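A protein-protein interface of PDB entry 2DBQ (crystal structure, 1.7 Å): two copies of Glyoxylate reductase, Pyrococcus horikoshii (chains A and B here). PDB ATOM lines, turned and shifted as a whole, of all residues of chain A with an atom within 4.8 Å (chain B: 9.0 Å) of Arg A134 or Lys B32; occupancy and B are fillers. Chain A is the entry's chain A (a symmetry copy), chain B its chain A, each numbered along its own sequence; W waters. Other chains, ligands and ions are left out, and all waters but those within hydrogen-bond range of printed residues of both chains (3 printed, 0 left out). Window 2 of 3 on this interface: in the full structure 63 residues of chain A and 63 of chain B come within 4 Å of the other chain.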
ATOM      1  N   PHE A 125      -5.320 -11.534  20.762  1.00  0.00           N
ATOM      2  CA  PHE A 125      -6.580 -11.082  21.349  1.00  0.00           C
ATOM      3  C   PHE A 125      -7.111 -12.071  22.392  1.00  0.00           C
ATOM      4  O   PHE A 125      -7.588 -11.679  23.460  1.00  0.00           O
ATOM      5  CB  PHE A 125      -7.609 -10.893  20.230  1.00  0.00           C
ATOM      6  CG  PHE A 125      -8.948 -10.406  20.701  1.00  0.00           C
ATOM      7  CD1 PHE A 125      -9.074  -9.167  21.328  1.00  0.00           C
ATOM      8  CD2 PHE A 125     -10.091 -11.168  20.481  1.00  0.00           C
ATOM      9  CE1 PHE A 125     -10.323  -8.692  21.727  1.00  0.00           C
ATOM     10  CE2 PHE A 125     -11.347 -10.706  20.874  1.00  0.00           C
ATOM     11  CZ  PHE A 125     -11.466  -9.465  21.498  1.00  0.00           C
ATOM     12  N   GLU A 130      -7.698 -10.312  26.529  1.00  0.00           N
ATOM     13  CA  GLU A 130      -8.506  -9.176  26.084  1.00  0.00           C
ATOM     14  C   GLU A 130      -9.913  -9.612  25.711  1.00  0.00           C
ATOM     15  O   GLU A 130     -10.887  -8.919  26.001  1.00  0.00           O
ATOM     16  CB  GLU A 130      -7.869  -8.506  24.871  1.00  0.00           C
ATOM     17  CG  GLU A 130      -6.603  -7.730  25.166  1.00  0.00           C
ATOM     18  CD  GLU A 130      -5.800  -7.458  23.907  1.00  0.00           C
ATOM     19  OE1 GLU A 130      -6.412  -7.071  22.884  1.00  0.00           O
ATOM     20  OE2 GLU A 130      -4.560  -7.631  23.941  1.00  0.00           O
ATOM     21  N   TRP A 131     -10.011 -10.762  25.054  1.00  0.00           N
ATOM     22  CA  TRP A 131     -11.303 -11.292  24.639  1.00  0.00           C
ATOM     23  C   TRP A 131     -12.229 -11.439  25.844  1.00  0.00           C
ATOM     24  O   TRP A 131     -13.350 -10.937  25.842  1.00  0.00           O
ATOM     25  CB  TRP A 131     -11.097 -12.647  23.954  1.00  0.00           C
ATOM     26  CG  TRP A 131     -12.315 -13.213  23.296  1.00  0.00           C
ATOM     27  CD1 TRP A 131     -13.372 -12.517  22.767  1.00  0.00           C
ATOM     28  CD2 TRP A 131     -12.557 -14.594  23.001  1.00  0.00           C
ATOM     29  NE1 TRP A 131     -14.252 -13.383  22.157  1.00  0.00           N
ATOM     30  CE2 TRP A 131     -13.776 -14.663  22.285  1.00  0.00           C
ATOM     31  CE3 TRP A 131     -11.859 -15.782  23.270  1.00  0.00           C
ATOM     32  CZ2 TRP A 131     -14.311 -15.877  21.832  1.00  0.00           C
ATOM     33  CZ3 TRP A 131     -12.393 -16.991  22.820  1.00  0.00           C
ATOM     34  CH2 TRP A 131     -13.609 -17.025  22.107  1.00  0.00           C
ATOM     35  N   LYS A 132     -11.746 -12.123  26.875  1.00  0.00           N
ATOM     36  CA  LYS A 132     -12.522 -12.342  28.089  1.00  0.00           C
ATOM     37  C   LYS A 132     -12.782 -11.043  28.859  1.00  0.00           C
ATOM     38  O   LYS A 132     -13.922 -10.740  29.216  1.00  0.00           O
ATOM     39  CB  LYS A 132     -11.784 -13.334  28.991  1.00  0.00           C
ATOM     40  CG  LYS A 132     -12.477 -13.645  30.305  1.00  0.00           C
ATOM     41  CD  LYS A 132     -13.799 -14.352  30.096  1.00  0.00           C
ATOM     42  CE  LYS A 132     -14.433 -14.714  31.431  1.00  0.00           C
ATOM     43  NZ  LYS A 132     -15.741 -15.401  31.254  1.00  0.00           N
ATOM     44  N   LYS A 133     -11.722 -10.277  29.101  1.00  0.00           N
ATOM     45  CA  LYS A 133     -11.821  -9.023  29.843  1.00  0.00           C
ATOM     46  C   LYS A 133     -12.875  -8.058  29.305  1.00  0.00           C
ATOM     47  O   LYS A 133     -13.596  -7.425  30.077  1.00  0.00           O
ATOM     48  CB  LYS A 133     -10.464  -8.318  29.872  1.00  0.00           C
ATOM     49  CG  LYS A 133     -10.480  -6.987  30.608  1.00  0.00           C
ATOM     50  CD  LYS A 133      -9.143  -6.270  30.491  1.00  0.00           C
ATOM     51  CE  LYS A 133      -9.134  -4.968  31.286  1.00  0.00           C
ATOM     52  NZ  LYS A 133      -7.840  -4.234  31.142  1.00  0.00           N
ATOM     53  N   ARG A 134     -12.964  -7.942  27.988  1.00  0.00           N
ATOM     54  CA  ARG A 134     -13.927  -7.042  27.379  1.00  0.00           C
ATOM     55  C   ARG A 134     -15.342  -7.600  27.414  1.00  0.00           C
ATOM     56  O   ARG A 134     -16.307  -6.884  27.161  1.00  0.00           O
ATOM     57  CB  ARG A 134     -13.484  -6.715  25.957  1.00  0.00           C
ATOM     58  CG  ARG A 134     -12.163  -5.965  25.965  1.00  0.00           C
ATOM     59  CD  ARG A 134     -11.575  -5.754  24.585  1.00  0.00           C
ATOM     60  NE  ARG A 134     -10.259  -5.126  24.689  1.00  0.00           N
ATOM     61  CZ  ARG A 134      -9.398  -5.003  23.683  1.00  0.00           C
ATOM     62  NH1 ARG A 134      -9.704  -5.466  22.476  1.00  0.00           N
ATOM     63  NH2 ARG A 134      -8.223  -4.424  23.889  1.00  0.00           N
ATOM     64  N   GLY A 135     -15.459  -8.885  27.730  1.00  0.00           N
ATOM     65  CA  GLY A 135     -16.768  -9.505  27.849  1.00  0.00           C
ATOM     66  C   GLY A 135     -17.676  -9.637  26.639  1.00  0.00           C
ATOM     67  O   GLY A 135     -18.854  -9.948  26.801  1.00  0.00           O
ATOM     68  N   VAL A 136     -17.160  -9.399  25.437  1.00  0.00           N
ATOM     69  CA  VAL A 136     -17.975  -9.544  24.232  1.00  0.00           C
ATOM     70  C   VAL A 136     -17.549 -10.832  23.530  1.00  0.00           C
ATOM     71  O   VAL A 136     -16.369 -11.026  23.238  1.00  0.00           O
ATOM     72  CB  VAL A 136     -17.793  -8.352  23.265  1.00  0.00           C
ATOM     73  CG1 VAL A 136     -18.636  -8.568  22.004  1.00  0.00           C
ATOM     74  CG2 VAL A 136     -18.195  -7.055  23.961  1.00  0.00           C
ATOM     75  N   THR B   8     -30.620 -10.178  16.379  1.00  0.00           N
ATOM     76  CA  THR B   8     -29.805  -9.957  17.576  1.00  0.00           C
ATOM     77  C   THR B   8     -28.374  -9.432  17.438  1.00  0.00           C
ATOM     78  O   THR B   8     -27.652  -9.317  18.436  1.00  0.00           O
ATOM     79  CB  THR B   8     -29.768 -11.235  18.433  1.00  0.00           C
ATOM     80  OG1 THR B   8     -29.064 -12.262  17.728  1.00  0.00           O
ATOM     81  CG2 THR B   8     -31.191 -11.717  18.724  1.00  0.00           C
ATOM     82  N   ARG B   9     -27.962  -9.110  16.215  1.00  0.00           N
ATOM     83  CA  ARG B   9     -26.621  -8.575  15.974  1.00  0.00           C
ATOM     84  C   ARG B   9     -26.623  -7.868  14.626  1.00  0.00           C
ATOM     85  O   ARG B   9     -27.431  -8.189  13.755  1.00  0.00           O
ATOM     86  CB  ARG B   9     -25.570  -9.697  15.958  1.00  0.00           C
ATOM     87  CG  ARG B   9     -24.274  -9.376  16.715  1.00  0.00           C
ATOM     88  CD  ARG B   9     -24.471  -9.573  18.211  1.00  0.00           C
ATOM     89  NE  ARG B   9     -23.238  -9.455  18.988  1.00  0.00           N
ATOM     90  CZ  ARG B   9     -22.836  -8.346  19.607  1.00  0.00           C
ATOM     91  NH1 ARG B   9     -23.564  -7.236  19.540  1.00  0.00           N
ATOM     92  NH2 ARG B   9     -21.720  -8.355  20.330  1.00  0.00           N
ATOM     93  N   GLU B  10     -25.722  -6.906  14.456  1.00  0.00           N
ATOM     94  CA  GLU B  10     -25.638  -6.164  13.208  1.00  0.00           C
ATOM     95  C   GLU B  10     -24.936  -6.944  12.105  1.00  0.00           C
ATOM     96  O   GLU B  10     -23.756  -6.728  11.825  1.00  0.00           O
ATOM     97  CB  GLU B  10     -24.930  -4.829  13.431  1.00  0.00           C
ATOM     98  CG  GLU B  10     -25.817  -3.788  14.070  1.00  0.00           C
ATOM     99  CD  GLU B  10     -25.182  -2.417  14.074  1.00  0.00           C
ATOM    100  OE1 GLU B  10     -24.291  -2.160  14.917  1.00  0.00           O
ATOM    101  OE2 GLU B  10     -25.572  -1.596  13.217  1.00  0.00           O
ATOM    102  N   TRP B  28     -30.424  -5.326  16.939  1.00  0.00           N
ATOM    103  CA  TRP B  28     -29.679  -5.039  18.160  1.00  0.00           C
ATOM    104  C   TRP B  28     -28.308  -4.490  17.758  1.00  0.00           C
ATOM    105  O   TRP B  28     -27.568  -5.131  17.012  1.00  0.00           O
ATOM    106  CB  TRP B  28     -29.530  -6.320  18.988  1.00  0.00           C
ATOM    107  CG  TRP B  28     -28.737  -6.154  20.253  1.00  0.00           C
ATOM    108  CD1 TRP B  28     -27.443  -6.537  20.468  1.00  0.00           C
ATOM    109  CD2 TRP B  28     -29.191  -5.568  21.480  1.00  0.00           C
ATOM    110  NE1 TRP B  28     -27.062  -6.229  21.754  1.00  0.00           N
ATOM    111  CE2 TRP B  28     -28.116  -5.633  22.397  1.00  0.00           C
ATOM    112  CE3 TRP B  28     -30.401  -4.991  21.894  1.00  0.00           C
ATOM    113  CZ2 TRP B  28     -28.217  -5.144  23.704  1.00  0.00           C
ATOM    114  CZ3 TRP B  28     -30.498  -4.505  23.191  1.00  0.00           C
ATOM    115  CH2 TRP B  28     -29.413  -4.585  24.080  1.00  0.00           C
ATOM    116  N   GLY B  29     -27.971  -3.301  18.251  1.00  0.00           N
ATOM    117  CA  GLY B  29     -26.696  -2.707  17.885  1.00  0.00           C
ATOM    118  C   GLY B  29     -25.746  -2.346  19.011  1.00  0.00           C
ATOM    119  O   GLY B  29     -24.860  -1.514  18.829  1.00  0.00           O
ATOM    120  N   ASP B  30     -25.910  -2.960  20.175  1.00  0.00           N
ATOM    121  CA  ASP B  30     -25.024  -2.658  21.285  1.00  0.00           C
ATOM    122  C   ASP B  30     -23.698  -3.395  21.114  1.00  0.00           C
ATOM    123  O   ASP B  30     -23.607  -4.372  20.371  1.00  0.00           O
ATOM    124  CB  ASP B  30     -25.683  -3.053  22.608  1.00  0.00           C
ATOM    125  CG  ASP B  30     -25.031  -2.383  23.803  1.00  0.00           C
ATOM    126  OD1 ASP B  30     -23.940  -2.824  24.223  1.00  0.00           O
ATOM    127  OD2 ASP B  30     -25.607  -1.402  24.314  1.00  0.00           O
ATOM    128  N   GLU B  31     -22.666  -2.914  21.795  1.00  0.00           N
ATOM    129  CA  GLU B  31     -21.345  -3.533  21.732  1.00  0.00           C
ATOM    130  C   GLU B  31     -21.401  -4.976  22.245  1.00  0.00           C
ATOM    131  O   GLU B  31     -20.843  -5.888  21.629  1.00  0.00           O
ATOM    132  CB  GLU B  31     -20.360  -2.705  22.567  1.00  0.00           C
ATOM    133  CG  GLU B  31     -18.968  -3.305  22.756  1.00  0.00           C
ATOM    134  CD  GLU B  31     -18.220  -3.510  21.449  1.00  0.00           C
ATOM    135  OE1 GLU B  31     -18.557  -2.827  20.452  1.00  0.00           O
ATOM    136  OE2 GLU B  31     -17.284  -4.345  21.428  1.00  0.00           O
ATOM    137  N   LYS B  32     -22.091  -5.181  23.364  1.00  0.00           N
ATOM    138  CA  LYS B  32     -22.209  -6.508  23.957  1.00  0.00           C
ATOM    139  C   LYS B  32     -23.428  -7.286  23.468  1.00  0.00           C
ATOM    140  O   LYS B  32     -24.364  -6.705  22.915  1.00  0.00           O
ATOM    141  CB  LYS B  32     -22.259  -6.392  25.481  1.00  0.00           C
ATOM    142  CG  LYS B  32     -20.985  -5.829  26.071  1.00  0.00           C
ATOM    143  CD  LYS B  32     -21.028  -5.796  27.580  1.00  0.00           C
ATOM    144  CE  LYS B  32     -19.739  -5.203  28.139  1.00  0.00           C
ATOM    145  NZ  LYS B  32     -19.807  -5.028  29.622  1.00  0.00           N
ATOM    146  N   GLU B  33     -23.397  -8.602  23.667  1.00  0.00           N
ATOM    147  CA  GLU B  33     -24.504  -9.473  23.278  1.00  0.00           C
ATOM    148  C   GLU B  33     -25.763  -9.015  24.005  1.00  0.00           C
ATOM    149  O   GLU B  33     -25.696  -8.505  25.124  1.00  0.00           O
ATOM    150  CB  GLU B  33     -24.216 -10.929  23.661  1.00  0.00           C
ATOM    151  CG  GLU B  33     -23.380 -11.718  22.658  1.00  0.00           C
ATOM    152  CD  GLU B  33     -21.961 -11.205  22.526  1.00  0.00           C
ATOM    153  OE1 GLU B  33     -21.339 -10.903  23.569  1.00  0.00           O
ATOM    154  OE2 GLU B  33     -21.462 -11.120  21.382  1.00  0.00           O
ATOM    155  N   ILE B  34     -26.914  -9.205  23.379  1.00  0.00           N
ATOM    156  CA  ILE B  34     -28.156  -8.784  23.998  1.00  0.00           C
ATOM    157  C   ILE B  34     -28.389  -9.517  25.325  1.00  0.00           C
ATOM    158  O   ILE B  34     -28.290 -10.747  25.400  1.00  0.00           O
ATOM    159  CB  ILE B  34     -29.352  -9.009  23.039  1.00  0.00           C
ATOM    160  CG1 ILE B  34     -30.627  -8.451  23.669  1.00  0.00           C
ATOM    161  CG2 ILE B  34     -29.499 -10.501  22.702  1.00  0.00           C
ATOM    162  CD1 ILE B  34     -31.821  -8.466  22.743  1.00  0.00           C
ATOM    163  N   PRO B  35     -28.672  -8.759  26.401  1.00  0.00           N
ATOM    164  CA  PRO B  35     -28.913  -9.366  27.710  1.00  0.00           C
ATOM    165  C   PRO B  35     -30.152 -10.246  27.684  1.00  0.00           C
ATOM    166  O   PRO B  35     -31.128  -9.963  26.989  1.00  0.00           O
ATOM    167  CB  PRO B  35     -29.087  -8.158  28.627  1.00  0.00           C
ATOM    168  CG  PRO B  35     -28.209  -7.127  27.982  1.00  0.00           C
ATOM    169  CD  PRO B  35     -28.558  -7.295  26.523  1.00  0.00           C
ATOM    170  N   ILE B  38     -33.449  -8.565  28.239  1.00  0.00           N
ATOM    171  CA  ILE B  38     -33.918  -7.776  27.106  1.00  0.00           C
ATOM    172  C   ILE B  38     -34.392  -8.686  25.973  1.00  0.00           C
ATOM    173  O   ILE B  38     -35.353  -8.367  25.270  1.00  0.00           O
ATOM    174  CB  ILE B  38     -32.821  -6.811  26.602  1.00  0.00           C
ATOM    175  CG1 ILE B  38     -32.448  -5.838  27.724  1.00  0.00           C
ATOM    176  CG2 ILE B  38     -33.317  -6.033  25.378  1.00  0.00           C
ATOM    177  CD1 ILE B  38     -31.371  -4.832  27.358  1.00  0.00           C
ATOM    178  N   SER B  54     -24.630 -16.820  20.540  1.00  0.00           N
ATOM    179  CA  SER B  54     -24.670 -16.237  21.876  1.00  0.00           C
ATOM    180  C   SER B  54     -26.062 -16.243  22.519  1.00  0.00           C
ATOM    181  O   SER B  54     -26.194 -16.062  23.737  1.00  0.00           O
ATOM    182  CB  SER B  54     -24.131 -14.805  21.828  1.00  0.00           C
ATOM    183  OG  SER B  54     -24.834 -14.021  20.878  1.00  0.00           O
ATOM    184  N   GLU B  55     -27.100 -16.438  21.707  1.00  0.00           N
ATOM    185  CA  GLU B  55     -28.465 -16.474  22.219  1.00  0.00           C
ATOM    186  C   GLU B  55     -28.953 -17.911  22.386  1.00  0.00           C
ATOM    187  O   GLU B  55     -28.992 -18.682  21.421  1.00  0.00           O
ATOM    188  CB  GLU B  55     -29.416 -15.709  21.291  1.00  0.00           C
ATOM    189  CG  GLU B  55     -29.288 -14.187  21.373  1.00  0.00           C
ATOM    190  CD  GLU B  55     -28.044 -13.665  20.691  1.00  0.00           C
ATOM    191  OE1 GLU B  55     -27.938 -13.844  19.459  1.00  0.00           O
ATOM    192  OE2 GLU B  55     -27.179 -13.083  21.383  1.00  0.00           O
ATOM    193  N   PRO B 271     -16.737 -15.458  25.456  1.00  0.00           N
ATOM    194  CA  PRO B 271     -15.270 -15.425  25.462  1.00  0.00           C
ATOM    195  C   PRO B 271     -14.660 -16.414  26.451  1.00  0.00           C
ATOM    196  O   PRO B 271     -15.307 -16.825  27.412  1.00  0.00           O
ATOM    197  CB  PRO B 271     -14.961 -13.969  25.804  1.00  0.00           C
ATOM    198  CG  PRO B 271     -16.112 -13.576  26.659  1.00  0.00           C
ATOM    199  CD  PRO B 271     -17.282 -14.169  25.912  1.00  0.00           C
ATOM    200  N   TYR B 272     -13.407 -16.787  26.208  1.00  0.00           N
ATOM    201  CA  TYR B 272     -12.719 -17.763  27.039  1.00  0.00           C
ATOM    202  C   TYR B 272     -11.400 -17.267  27.623  1.00  0.00           C
ATOM    203  O   TYR B 272     -10.716 -16.422  27.048  1.00  0.00           O
ATOM    204  CB  TYR B 272     -12.448 -19.019  26.204  1.00  0.00           C
ATOM    205  CG  TYR B 272     -11.953 -20.220  26.978  1.00  0.00           C
ATOM    206  CD1 TYR B 272     -12.768 -20.849  27.918  1.00  0.00           C
ATOM    207  CD2 TYR B 272     -10.683 -20.743  26.753  1.00  0.00           C
ATOM    208  CE1 TYR B 272     -12.333 -21.975  28.615  1.00  0.00           C
ATOM    209  CE2 TYR B 272     -10.236 -21.871  27.443  1.00  0.00           C
ATOM    210  CZ  TYR B 272     -11.068 -22.482  28.372  1.00  0.00           C
ATOM    211  OH  TYR B 272     -10.641 -23.602  29.056  1.00  0.00           O
HETATM  212  O   HOH W   1     -17.565 -16.271  28.975  1.00  0.00           O
HETATM  213  O   HOH W   2     -21.366  -9.562  25.795  1.00  0.00           O
HETATM  214  O   HOH W   3      -9.347 -14.167  26.598  1.00  0.00           O
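The backbone carbonyl oxygen of Phe A125 lies within hydrogen-bond range of the backbone NH of Trp A131. NH2 of Arg B9 is in hydrogen-bond range of O of Glu B31, at 2.9 Å. The side-chain carboxylate (OE1) of Glu A130 lies within salt-bridge range of the guanidinium group (NH2) of Arg A134 (3.4 Å). O of Asp B30 lies within hydrogen-bond range of NH1 of Arg B9, at 3.0 Å. The indole nitrogen (NE1) of Trp A131 sits at hydrogen-bond distance from the backbone carbonyl oxygen (O) of Val A136 (3.3 Å). The backbone carbonyl oxygen (O) of Lys B32 is in hydrogen-bond range of the indole nitrogen (NE1) of Trp B28 (3.0 Å).
Arg A134 touches just one residue of chain B: Lys B32. No residue of chain B comes within 4 Å of Gly A135. Printed residues of chain A within 4 Å of Arg B9: Val A136 (3.5 Å). Trp B28 touches none of the printed residues of chain A. Asp B30 touches none of the printed residues of chain A. Of the printed residues of chain A, Glu B31 touches Val A136. Lys B32 touches just these residues of chain A: Arg A134 (3.9 Å) and Val A136 (3.7 Å). The nearest residue of chain A that does not touch Lys B32 is Gly A135 (4.7 Å).
No position is printed for both chains. Of the 9 pairs that touch across the chains among the printed residues, none has its exchanged pair printed and touching as well.
Water W2 lies within hydrogen-bond range of OE1 of Glu B33 and O of Gly A135. Water W3 bridges O of Tyr B272 (2.7 Å) and N of Lys A132 (3.2 Å). Water W1 bridges the backbone carbonyl oxygen of Pro B271 (2.8 Å) and the side-chain amino group of Lys A132 (3.0 Å).
Pro B271 touches Trp A131. Trp A131 touches Tyr B272 (CE3 to N, 3.5 Å). Lys A132 touches Pro B271. Tyr B272 touches Lys A132 (O to CB, 3.8 Å). Arg A134 touches Lys B32. Arg B9 touches Val A136. Val A136 touches Glu B31. Val A136 touches Lys B32. OE1 of Glu B33 touches CA of Val A136 (3.7 Å).
Of the 16 printed residues of chain B, 6 touch a printed residue of chain A. Printed residues of chain B that touch a printed residue of chain A: Arg B9, Glu B31, Lys B32, Glu B33, Pro B271 and Tyr B272. Hydrophobic or aromatic side chains of chain B within 4 Å of the printed part of chain A: Pro B271 and Tyr B272. Along chain B the printed residues that touch a printed residue of chain A span positions 9 to 272. Printed residues of chain A that touch a printed residue of chain B: Trp A131, Lys A132, Arg A134 and Val A136. Hydrophobic or aromatic side chains of chain A within 4 Å of the printed part of chain B: Trp A131 and Val A136. Among the printed residues, 9 pairs touch across the chains. Among the printed residues, no Asp or Glu carboxylate lies within 4 Å of a Lys or Arg side-chain nitrogen of the other chain.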
